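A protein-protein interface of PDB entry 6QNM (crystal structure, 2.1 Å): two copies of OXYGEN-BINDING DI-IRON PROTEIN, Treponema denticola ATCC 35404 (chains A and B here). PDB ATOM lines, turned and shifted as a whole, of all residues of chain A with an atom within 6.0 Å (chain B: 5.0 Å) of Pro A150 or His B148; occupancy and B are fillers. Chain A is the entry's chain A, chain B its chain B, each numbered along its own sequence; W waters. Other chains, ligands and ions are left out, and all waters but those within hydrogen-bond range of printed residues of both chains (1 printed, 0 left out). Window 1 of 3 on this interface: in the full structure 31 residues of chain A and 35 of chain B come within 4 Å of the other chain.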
ATOM      1  N   GLN A  81     -12.701   8.103 -20.281  1.00  0.00           N
ATOM      2  CA  GLN A  81     -11.535   8.169 -21.141  1.00  0.00           C
ATOM      3  C   GLN A  81     -11.716   9.396 -22.020  1.00  0.00           C
ATOM      4  O   GLN A  81     -12.824   9.681 -22.484  1.00  0.00           O
ATOM      5  CB  GLN A  81     -11.383   6.883 -21.963  1.00  0.00           C
ATOM      6  CG  GLN A  81     -11.992   6.881 -23.373  1.00  0.00           C
ATOM      7  CD  GLN A  81     -13.517   6.881 -23.384  1.00  0.00           C
ATOM      8  OE1 GLN A  81     -14.170   7.080 -22.356  1.00  0.00           O
ATOM      9  NE2 GLN A  81     -14.093   6.653 -24.561  1.00  0.00           N
ATOM     10  N   SER A 103     -12.754   4.212 -14.778  1.00  0.00           N
ATOM     11  CA  SER A 103     -13.622   3.065 -15.003  1.00  0.00           C
ATOM     12  C   SER A 103     -12.811   1.864 -15.471  1.00  0.00           C
ATOM     13  O   SER A 103     -11.833   2.003 -16.212  1.00  0.00           O
ATOM     14  CB  SER A 103     -14.697   3.411 -16.039  1.00  0.00           C
ATOM     15  OG  SER A 103     -15.332   2.242 -16.537  1.00  0.00           O
ATOM     16  N   LEU A 105     -13.571  -0.142 -17.622  1.00  0.00           N
ATOM     17  CA  LEU A 105     -13.693  -0.277 -19.073  1.00  0.00           C
ATOM     18  C   LEU A 105     -12.467   0.251 -19.811  1.00  0.00           C
ATOM     19  O   LEU A 105     -12.186  -0.180 -20.935  1.00  0.00           O
ATOM     20  CB  LEU A 105     -14.947   0.449 -19.566  1.00  0.00           C
ATOM     21  CG  LEU A 105     -16.231  -0.383 -19.664  1.00  0.00           C
ATOM     22  CD1 LEU A 105     -16.689  -0.845 -18.287  1.00  0.00           C
ATOM     23  CD2 LEU A 105     -17.330   0.404 -20.357  1.00  0.00           C
ATOM     24  N   TRP A 106     -11.762   1.220 -19.232  1.00  0.00           N
ATOM     25  CA  TRP A 106     -10.669   1.893 -19.916  1.00  0.00           C
ATOM     26  C   TRP A 106      -9.279   1.493 -19.439  1.00  0.00           C
ATOM     27  O   TRP A 106      -8.297   1.862 -20.093  1.00  0.00           O
ATOM     28  CB  TRP A 106     -10.845   3.412 -19.795  1.00  0.00           C
ATOM     29  CG  TRP A 106     -12.236   3.830 -20.162  1.00  0.00           C
ATOM     30  CD1 TRP A 106     -13.115   4.530 -19.387  1.00  0.00           C
ATOM     31  CD2 TRP A 106     -12.918   3.551 -21.391  1.00  0.00           C
ATOM     32  NE1 TRP A 106     -14.298   4.711 -20.061  1.00  0.00           N
ATOM     33  CE2 TRP A 106     -14.202   4.122 -21.294  1.00  0.00           C
ATOM     34  CE3 TRP A 106     -12.564   2.880 -22.569  1.00  0.00           C
ATOM     35  CZ2 TRP A 106     -15.136   4.038 -22.325  1.00  0.00           C
ATOM     36  CZ3 TRP A 106     -13.493   2.799 -23.593  1.00  0.00           C
ATOM     37  CH2 TRP A 106     -14.763   3.375 -23.464  1.00  0.00           C
ATOM     38  N   ASP A 126     -18.392  -1.029 -12.134  1.00  0.00           N
ATOM     39  CA  ASP A 126     -19.499  -0.355 -12.810  1.00  0.00           C
ATOM     40  C   ASP A 126     -20.449   0.331 -11.835  1.00  0.00           C
ATOM     41  O   ASP A 126     -20.965   1.417 -12.124  1.00  0.00           O
ATOM     42  CB  ASP A 126     -20.258  -1.359 -13.680  1.00  0.00           C
ATOM     43  CG  ASP A 126     -19.567  -1.612 -15.010  1.00  0.00           C
ATOM     44  OD1 ASP A 126     -18.727  -0.777 -15.410  1.00  0.00           O
ATOM     45  OD2 ASP A 126     -19.855  -2.644 -15.650  1.00  0.00           O
ATOM     46  N   HIS A 145     -22.694   5.961 -16.606  1.00  0.00           N
ATOM     47  CA  HIS A 145     -22.408   5.296 -17.866  1.00  0.00           C
ATOM     48  C   HIS A 145     -23.373   5.733 -18.960  1.00  0.00           C
ATOM     49  O   HIS A 145     -24.553   6.003 -18.712  1.00  0.00           O
ATOM     50  CB  HIS A 145     -22.468   3.784 -17.665  1.00  0.00           C
ATOM     51  CG  HIS A 145     -21.625   3.312 -16.525  1.00  0.00           C
ATOM     52  ND1 HIS A 145     -20.259   3.494 -16.495  1.00  0.00           N
ATOM     53  CD2 HIS A 145     -21.948   2.682 -15.371  1.00  0.00           C
ATOM     54  CE1 HIS A 145     -19.775   2.984 -15.377  1.00  0.00           C
ATOM     55  NE2 HIS A 145     -20.779   2.484 -14.678  1.00  0.00           N
ATOM     56  N   PHE A 146     -22.843   5.805 -20.184  1.00  0.00           N
ATOM     57  CA  PHE A 146     -23.595   6.175 -21.386  1.00  0.00           C
ATOM     58  C   PHE A 146     -24.101   7.614 -21.322  1.00  0.00           C
ATOM     59  O   PHE A 146     -25.109   7.960 -21.945  1.00  0.00           O
ATOM     60  CB  PHE A 146     -24.743   5.197 -21.648  1.00  0.00           C
ATOM     61  CG  PHE A 146     -24.273   3.801 -21.931  1.00  0.00           C
ATOM     62  CD1 PHE A 146     -23.702   3.485 -23.157  1.00  0.00           C
ATOM     63  CD2 PHE A 146     -24.367   2.814 -20.964  1.00  0.00           C
ATOM     64  CE1 PHE A 146     -23.249   2.210 -23.417  1.00  0.00           C
ATOM     65  CE2 PHE A 146     -23.917   1.527 -21.223  1.00  0.00           C
ATOM     66  CZ  PHE A 146     -23.357   1.230 -22.451  1.00  0.00           C
ATOM     67  N   MET A 147     -23.398   8.469 -20.578  1.00  0.00           N
ATOM     68  CA  MET A 147     -23.703   9.897 -20.532  1.00  0.00           C
ATOM     69  C   MET A 147     -22.426  10.743 -20.611  1.00  0.00           C
ATOM     70  O   MET A 147     -22.142  11.564 -19.744  1.00  0.00           O
ATOM     71  CB  MET A 147     -24.489  10.224 -19.262  1.00  0.00           C
ATOM     72  CG  MET A 147     -25.892   9.637 -19.237  1.00  0.00           C
ATOM     73  SD  MET A 147     -26.659   9.703 -17.611  1.00  0.00           S
ATOM     74  CE  MET A 147     -26.647  11.470 -17.300  1.00  0.00           C
ATOM     75  N   HIS A 148     -21.642  10.600 -21.683  1.00  0.00           N
ATOM     76  CA  HIS A 148     -21.977   9.832 -22.877  1.00  0.00           C
ATOM     77  C   HIS A 148     -21.158   8.545 -23.014  1.00  0.00           C
ATOM     78  O   HIS A 148     -21.528   7.641 -23.768  1.00  0.00           O
ATOM     79  CB  HIS A 148     -21.764  10.696 -24.115  1.00  0.00           C
ATOM     80  CG  HIS A 148     -20.388  11.281 -24.211  1.00  0.00           C
ATOM     81  ND1 HIS A 148     -19.308  10.569 -24.686  1.00  0.00           N
ATOM     82  CD2 HIS A 148     -19.915  12.509 -23.888  1.00  0.00           C
ATOM     83  CE1 HIS A 148     -18.231  11.332 -24.655  1.00  0.00           C
ATOM     84  NE2 HIS A 148     -18.572  12.514 -24.174  1.00  0.00           N
ATOM     85  N   SER A 149     -20.051   8.460 -22.286  1.00  0.00           N
ATOM     86  CA  SER A 149     -19.143   7.334 -22.469  1.00  0.00           C
ATOM     87  C   SER A 149     -19.722   6.078 -21.818  1.00  0.00           C
ATOM     88  O   SER A 149     -20.397   6.167 -20.789  1.00  0.00           O
ATOM     89  CB  SER A 149     -17.774   7.657 -21.872  1.00  0.00           C
ATOM     90  OG  SER A 149     -16.934   6.517 -21.848  1.00  0.00           O
ATOM     91  N   PRO A 150     -19.500   4.897 -22.407  1.00  0.00           N
ATOM     92  CA  PRO A 150     -20.045   3.669 -21.805  1.00  0.00           C
ATOM     93  C   PRO A 150     -19.475   3.373 -20.431  1.00  0.00           C
ATOM     94  O   PRO A 150     -20.130   2.679 -19.642  1.00  0.00           O
ATOM     95  CB  PRO A 150     -19.669   2.577 -22.820  1.00  0.00           C
ATOM     96  CG  PRO A 150     -18.543   3.148 -23.606  1.00  0.00           C
ATOM     97  CD  PRO A 150     -18.795   4.626 -23.671  1.00  0.00           C
ATOM     98  N   GLY A 151     -18.280   3.872 -20.121  1.00  0.00           N
ATOM     99  CA  GLY A 151     -17.700   3.729 -18.799  1.00  0.00           C
ATOM    100  C   GLY A 151     -17.374   5.087 -18.218  1.00  0.00           C
ATOM    101  O   GLY A 151     -16.362   5.699 -18.570  1.00  0.00           O
ATOM    102  N   GLN A 152     -18.231   5.573 -17.323  1.00  0.00           N
ATOM    103  CA  GLN A 152     -18.172   6.969 -16.924  1.00  0.00           C
ATOM    104  C   GLN A 152     -18.644   7.125 -15.488  1.00  0.00           C
ATOM    105  O   GLN A 152     -19.610   6.476 -15.075  1.00  0.00           O
ATOM    106  CB  GLN A 152     -19.030   7.818 -17.866  1.00  0.00           C
ATOM    107  CG  GLN A 152     -19.189   9.267 -17.452  1.00  0.00           C
ATOM    108  CD  GLN A 152     -19.831  10.086 -18.546  1.00  0.00           C
ATOM    109  OE1 GLN A 152     -19.834   9.686 -19.712  1.00  0.00           O
ATOM    110  NE2 GLN A 152     -20.407  11.221 -18.177  1.00  0.00           N
ATOM    111  N   HIS B  80     -13.632   7.438 -34.922  1.00  0.00           N
ATOM    112  CA  HIS B  80     -14.137   8.221 -33.793  1.00  0.00           C
ATOM    113  C   HIS B  80     -12.977   8.914 -33.078  1.00  0.00           C
ATOM    114  O   HIS B  80     -11.819   8.836 -33.502  1.00  0.00           O
ATOM    115  CB  HIS B  80     -14.947   7.345 -32.831  1.00  0.00           C
ATOM    116  CG  HIS B  80     -14.136   6.302 -32.129  1.00  0.00           C
ATOM    117  ND1 HIS B  80     -13.570   6.509 -30.890  1.00  0.00           N
ATOM    118  CD2 HIS B  80     -13.810   5.037 -32.486  1.00  0.00           C
ATOM    119  CE1 HIS B  80     -12.923   5.418 -30.516  1.00  0.00           C
ATOM    120  NE2 HIS B  80     -13.054   4.511 -31.467  1.00  0.00           N
ATOM    121  N   PHE B 146     -22.966   5.715 -31.102  1.00  0.00           N
ATOM    122  CA  PHE B 146     -23.286   5.021 -29.851  1.00  0.00           C
ATOM    123  C   PHE B 146     -22.918   3.543 -29.905  1.00  0.00           C
ATOM    124  O   PHE B 146     -23.491   2.720 -29.186  1.00  0.00           O
ATOM    125  CB  PHE B 146     -24.757   5.213 -29.467  1.00  0.00           C
ATOM    126  CG  PHE B 146     -25.104   6.643 -29.134  1.00  0.00           C
ATOM    127  CD1 PHE B 146     -24.736   7.193 -27.915  1.00  0.00           C
ATOM    128  CD2 PHE B 146     -25.775   7.441 -30.049  1.00  0.00           C
ATOM    129  CE1 PHE B 146     -25.039   8.514 -27.608  1.00  0.00           C
ATOM    130  CE2 PHE B 146     -26.082   8.763 -29.750  1.00  0.00           C
ATOM    131  CZ  PHE B 146     -25.714   9.299 -28.527  1.00  0.00           C
ATOM    132  N   MET B 147     -21.927   3.200 -30.728  1.00  0.00           N
ATOM    133  CA  MET B 147     -21.406   1.843 -30.787  1.00  0.00           C
ATOM    134  C   MET B 147     -19.871   1.838 -30.811  1.00  0.00           C
ATOM    135  O   MET B 147     -19.244   1.264 -31.697  1.00  0.00           O
ATOM    136  CB  MET B 147     -21.972   1.122 -32.014  1.00  0.00           C
ATOM    137  CG  MET B 147     -23.464   0.813 -31.929  1.00  0.00           C
ATOM    138  SD  MET B 147     -24.202   0.230 -33.477  1.00  0.00           S
ATOM    139  CE  MET B 147     -23.263  -1.271 -33.756  1.00  0.00           C
ATOM    140  N   HIS B 148     -19.223   2.432 -29.802  1.00  0.00           N
ATOM    141  CA  HIS B 148     -19.843   2.953 -28.584  1.00  0.00           C
ATOM    142  C   HIS B 148     -19.838   4.488 -28.523  1.00  0.00           C
ATOM    143  O   HIS B 148     -20.582   5.083 -27.740  1.00  0.00           O
ATOM    144  CB  HIS B 148     -19.128   2.395 -27.354  1.00  0.00           C
ATOM    145  CG  HIS B 148     -17.647   2.615 -27.364  1.00  0.00           C
ATOM    146  ND1 HIS B 148     -17.068   3.803 -26.971  1.00  0.00           N
ATOM    147  CD2 HIS B 148     -16.625   1.797 -27.714  1.00  0.00           C
ATOM    148  CE1 HIS B 148     -15.755   3.708 -27.080  1.00  0.00           C
ATOM    149  NE2 HIS B 148     -15.460   2.501 -27.527  1.00  0.00           N
ATOM    150  N   SER B 149     -19.005   5.129 -29.359  1.00  0.00           N
ATOM    151  CA  SER B 149     -18.818   6.573 -29.255  1.00  0.00           C
ATOM    152  C   SER B 149     -20.029   7.318 -29.821  1.00  0.00           C
ATOM    153  O   SER B 149     -20.629   6.874 -30.804  1.00  0.00           O
ATOM    154  CB  SER B 149     -17.556   7.006 -29.998  1.00  0.00           C
ATOM    155  OG  SER B 149     -17.517   8.417 -30.160  1.00  0.00           O
ATOM    156  N   PRO B 150     -20.398   8.454 -29.220  1.00  0.00           N
ATOM    157  CA  PRO B 150     -21.579   9.191 -29.704  1.00  0.00           C
ATOM    158  C   PRO B 150     -21.438   9.705 -31.121  1.00  0.00           C
ATOM    159  O   PRO B 150     -22.453   9.926 -31.791  1.00  0.00           O
ATOM    160  CB  PRO B 150     -21.704  10.351 -28.704  1.00  0.00           C
ATOM    161  CG  PRO B 150     -20.949   9.904 -27.502  1.00  0.00           C
ATOM    162  CD  PRO B 150     -19.829   9.060 -28.005  1.00  0.00           C
ATOM    163  N   GLN B 152     -19.502   8.465 -34.449  1.00  0.00           N
ATOM    164  CA  GLN B 152     -18.679   7.369 -34.940  1.00  0.00           C
ATOM    165  C   GLN B 152     -19.158   6.934 -36.317  1.00  0.00           C
ATOM    166  O   GLN B 152     -20.361   6.937 -36.594  1.00  0.00           O
ATOM    167  CB  GLN B 152     -18.700   6.181 -33.966  1.00  0.00           C
ATOM    168  CG  GLN B 152     -17.911   4.973 -34.457  1.00  0.00           C
ATOM    169  CD  GLN B 152     -17.703   3.906 -33.398  1.00  0.00           C
ATOM    170  OE1 GLN B 152     -18.000   4.107 -32.217  1.00  0.00           O
ATOM    171  NE2 GLN B 152     -17.177   2.762 -33.818  1.00  0.00           N
ATOM    172  N   ASP B 167     -14.469  -0.225 -34.245  1.00  0.00           N
ATOM    173  CA  ASP B 167     -14.596  -1.054 -33.046  1.00  0.00           C
ATOM    174  C   ASP B 167     -15.666  -2.126 -33.186  1.00  0.00           C
ATOM    175  O   ASP B 167     -15.658  -3.097 -32.420  1.00  0.00           O
ATOM    176  CB  ASP B 167     -14.936  -0.192 -31.826  1.00  0.00           C
ATOM    177  CG  ASP B 167     -13.743   0.574 -31.290  1.00  0.00           C
ATOM    178  OD1 ASP B 167     -12.596   0.165 -31.567  1.00  0.00           O
ATOM    179  OD2 ASP B 167     -13.960   1.578 -30.577  1.00  0.00           O
ATOM    180  N   PHE B 195     -16.976  -7.309 -24.890  1.00  0.00           N
ATOM    181  CA  PHE B 195     -16.854  -5.928 -25.343  1.00  0.00           C
ATOM    182  C   PHE B 195     -18.185  -5.400 -25.868  1.00  0.00           C
ATOM    183  O   PHE B 195     -18.600  -4.287 -25.531  1.00  0.00           O
ATOM    184  CB  PHE B 195     -15.770  -5.831 -26.420  1.00  0.00           C
ATOM    185  CG  PHE B 195     -15.687  -4.482 -27.092  1.00  0.00           C
ATOM    186  CD1 PHE B 195     -15.269  -3.365 -26.388  1.00  0.00           C
ATOM    187  CD2 PHE B 195     -16.015  -4.338 -28.432  1.00  0.00           C
ATOM    188  CE1 PHE B 195     -15.186  -2.123 -27.009  1.00  0.00           C
ATOM    189  CE2 PHE B 195     -15.935  -3.102 -29.060  1.00  0.00           C
ATOM    190  CZ  PHE B 195     -15.520  -1.994 -28.350  1.00  0.00           C
ATOM    191  N   ARG B 198     -21.121  -4.961 -23.155  1.00  0.00           N
ATOM    192  CA  ARG B 198     -20.935  -3.881 -22.189  1.00  0.00           C
ATOM    193  C   ARG B 198     -20.759  -2.506 -22.834  1.00  0.00           C
ATOM    194  O   ARG B 198     -21.185  -1.502 -22.249  1.00  0.00           O
ATOM    195  CB  ARG B 198     -19.729  -4.183 -21.292  1.00  0.00           C
ATOM    196  CG  ARG B 198     -19.431  -3.116 -20.238  1.00  0.00           C
ATOM    197  CD  ARG B 198     -20.620  -2.858 -19.314  1.00  0.00           C
ATOM    198  NE  ARG B 198     -20.331  -1.802 -18.344  1.00  0.00           N
ATOM    199  CZ  ARG B 198     -20.441  -0.502 -18.601  1.00  0.00           C
ATOM    200  NH1 ARG B 198     -20.839  -0.094 -19.800  1.00  0.00           N
ATOM    201  NH2 ARG B 198     -20.156   0.394 -17.666  1.00  0.00           N
ATOM    202  N   TYR B 199     -20.162  -2.426 -24.022  1.00  0.00           N
ATOM    203  CA  TYR B 199     -19.824  -1.128 -24.603  1.00  0.00           C
ATOM    204  C   TYR B 199     -20.862  -0.609 -25.593  1.00  0.00           C
ATOM    205  O   TYR B 199     -21.059   0.609 -25.674  1.00  0.00           O
ATOM    206  CB  TYR B 199     -18.455  -1.186 -25.292  1.00  0.00           C
ATOM    207  CG  TYR B 199     -17.271  -1.365 -24.351  1.00  0.00           C
ATOM    208  CD1 TYR B 199     -17.106  -2.535 -23.617  1.00  0.00           C
ATOM    209  CD2 TYR B 199     -16.307  -0.371 -24.218  1.00  0.00           C
ATOM    210  CE1 TYR B 199     -16.021  -2.708 -22.763  1.00  0.00           C
ATOM    211  CE2 TYR B 199     -15.220  -0.534 -23.374  1.00  0.00           C
ATOM    212  CZ  TYR B 199     -15.081  -1.705 -22.650  1.00  0.00           C
ATOM    213  OH  TYR B 199     -14.005  -1.873 -21.809  1.00  0.00           O
ATOM    214  N   MET B 200     -21.511  -1.479 -26.367  1.00  0.00           N
ATOM    215  CA  MET B 200     -22.564  -1.022 -27.269  1.00  0.00           C
ATOM    216  C   MET B 200     -23.776  -0.562 -26.465  1.00  0.00           C
ATOM    217  O   MET B 200     -24.153  -1.190 -25.474  1.00  0.00           O
ATOM    218  CB  MET B 200     -22.967  -2.127 -28.248  1.00  0.00           C
ATOM    219  CG  MET B 200     -21.803  -2.760 -29.006  1.00  0.00           C
ATOM    220  SD  MET B 200     -21.008  -1.614 -30.151  1.00  0.00           S
ATOM    221  CE  MET B 200     -19.286  -1.841 -29.712  1.00  0.00           C
HETATM  222  O   HOH W   1     -22.165   5.882 -25.643  1.00  0.00           O
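The side-chain hydroxyl (OH) of Tyr B199 lies within hydrogen-bond range of the backbone carbonyl oxygen (O) of Leu A105, 2.6 Å away.
The side-chain carboxylate of Asp A126 lies within salt-bridge range of the guanidinium group of Arg B198, 2.9 Å away.
A ring nitrogen (ND1) of His A145 is in hydrogen-bond range of the guanidinium group of Arg B198.
The backbone carbonyl oxygen (O) of Pro A150 is in hydrogen-bond range of the guanidinium group (NH1) of Arg B198 (2.9 Å).
OE1 of Gln A81 sits close to NE1 of Trp A106, 3.3 Å away.
The backbone NH of Leu A105 lies close to the side-chain hydroxyl of Ser A103.
The indole nitrogen (NE1) of Trp A106 is in hydrogen-bond range of the backbone carbonyl oxygen (O) of Gly A151.
O of Asp A126 is in hydrogen-bond range of NE2 of His A145 (2.8 Å).
A ring nitrogen (ND1) of His A145 sits at hydrogen-bond distance from the backbone carbonyl oxygen (O) of Pro A150 (3.3 Å).
OE1 of Gln B152 is in hydrogen-bond range of N of His B148 (3.2 Å).
Water W1 bridges the backbone carbonyl oxygen (O) of His A148 (2.6 Å) and the backbone carbonyl oxygen (O) of His B148 (2.7 Å).
His A148 touches Pro B150, and with the chains exchanged Pro A150 touches His B148.
6 positions are printed for both chains.
Printed residues of chain B within 4 Å of Trp A106: His B148 and Tyr B199.
Of the printed residues of chain B, Asp A126 touches Arg B198 (2.9 Å).
His B148 touches just these residues of chain A: Trp A106 (3.8 Å) and Pro A150 (3.7 Å).
Of the printed residues of chain A, Arg B198 touches Leu A105, Asp A126, His A145, Phe A146 and Pro A150.
Of the printed residues of chain A, Met B200 touches Phe A146 (3.95 Å).
The nearest printed residue of chain B that does not touch Trp A106 is Phe B195 (6.2 Å).
Of the 13 printed residues of chain A, 7 touch a printed residue of chain B.
Hydrophobic or aromatic side chains of chain A within 4 Å of the printed part of chain B: Leu A105, Trp A106, His A145, Phe A146, His A148 and Pro A150.
Of the 12 printed residues of chain B, 5 touch a printed residue of chain A.
Among the printed residues, 13 pairs touch across the chains.
Among the printed residues, Asp or Glu carboxylates within 4 Å of a Lys or Arg side-chain nitrogen of the other chain: Asp A126 with Arg B198 (2.9 Å).
Arg B198 touches Leu A105.
CH2 of Trp A106 touches CE1 of His B148 (3.8 Å).
Trp A106 touches Tyr B199.
O of Arg B198 touches CZ of Phe A146 (3.5 Å).
CE1 of Phe A146 touches O of Tyr B199, 3.5 Å away.
Phe A146 touches Met B200.
His A148 touches Pro B150 (ND1 to CG, 3.3 Å).
Pro A150 touches His B148 (CG to ND1, 3.7 Å).
Pro A150 touches Tyr B199.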
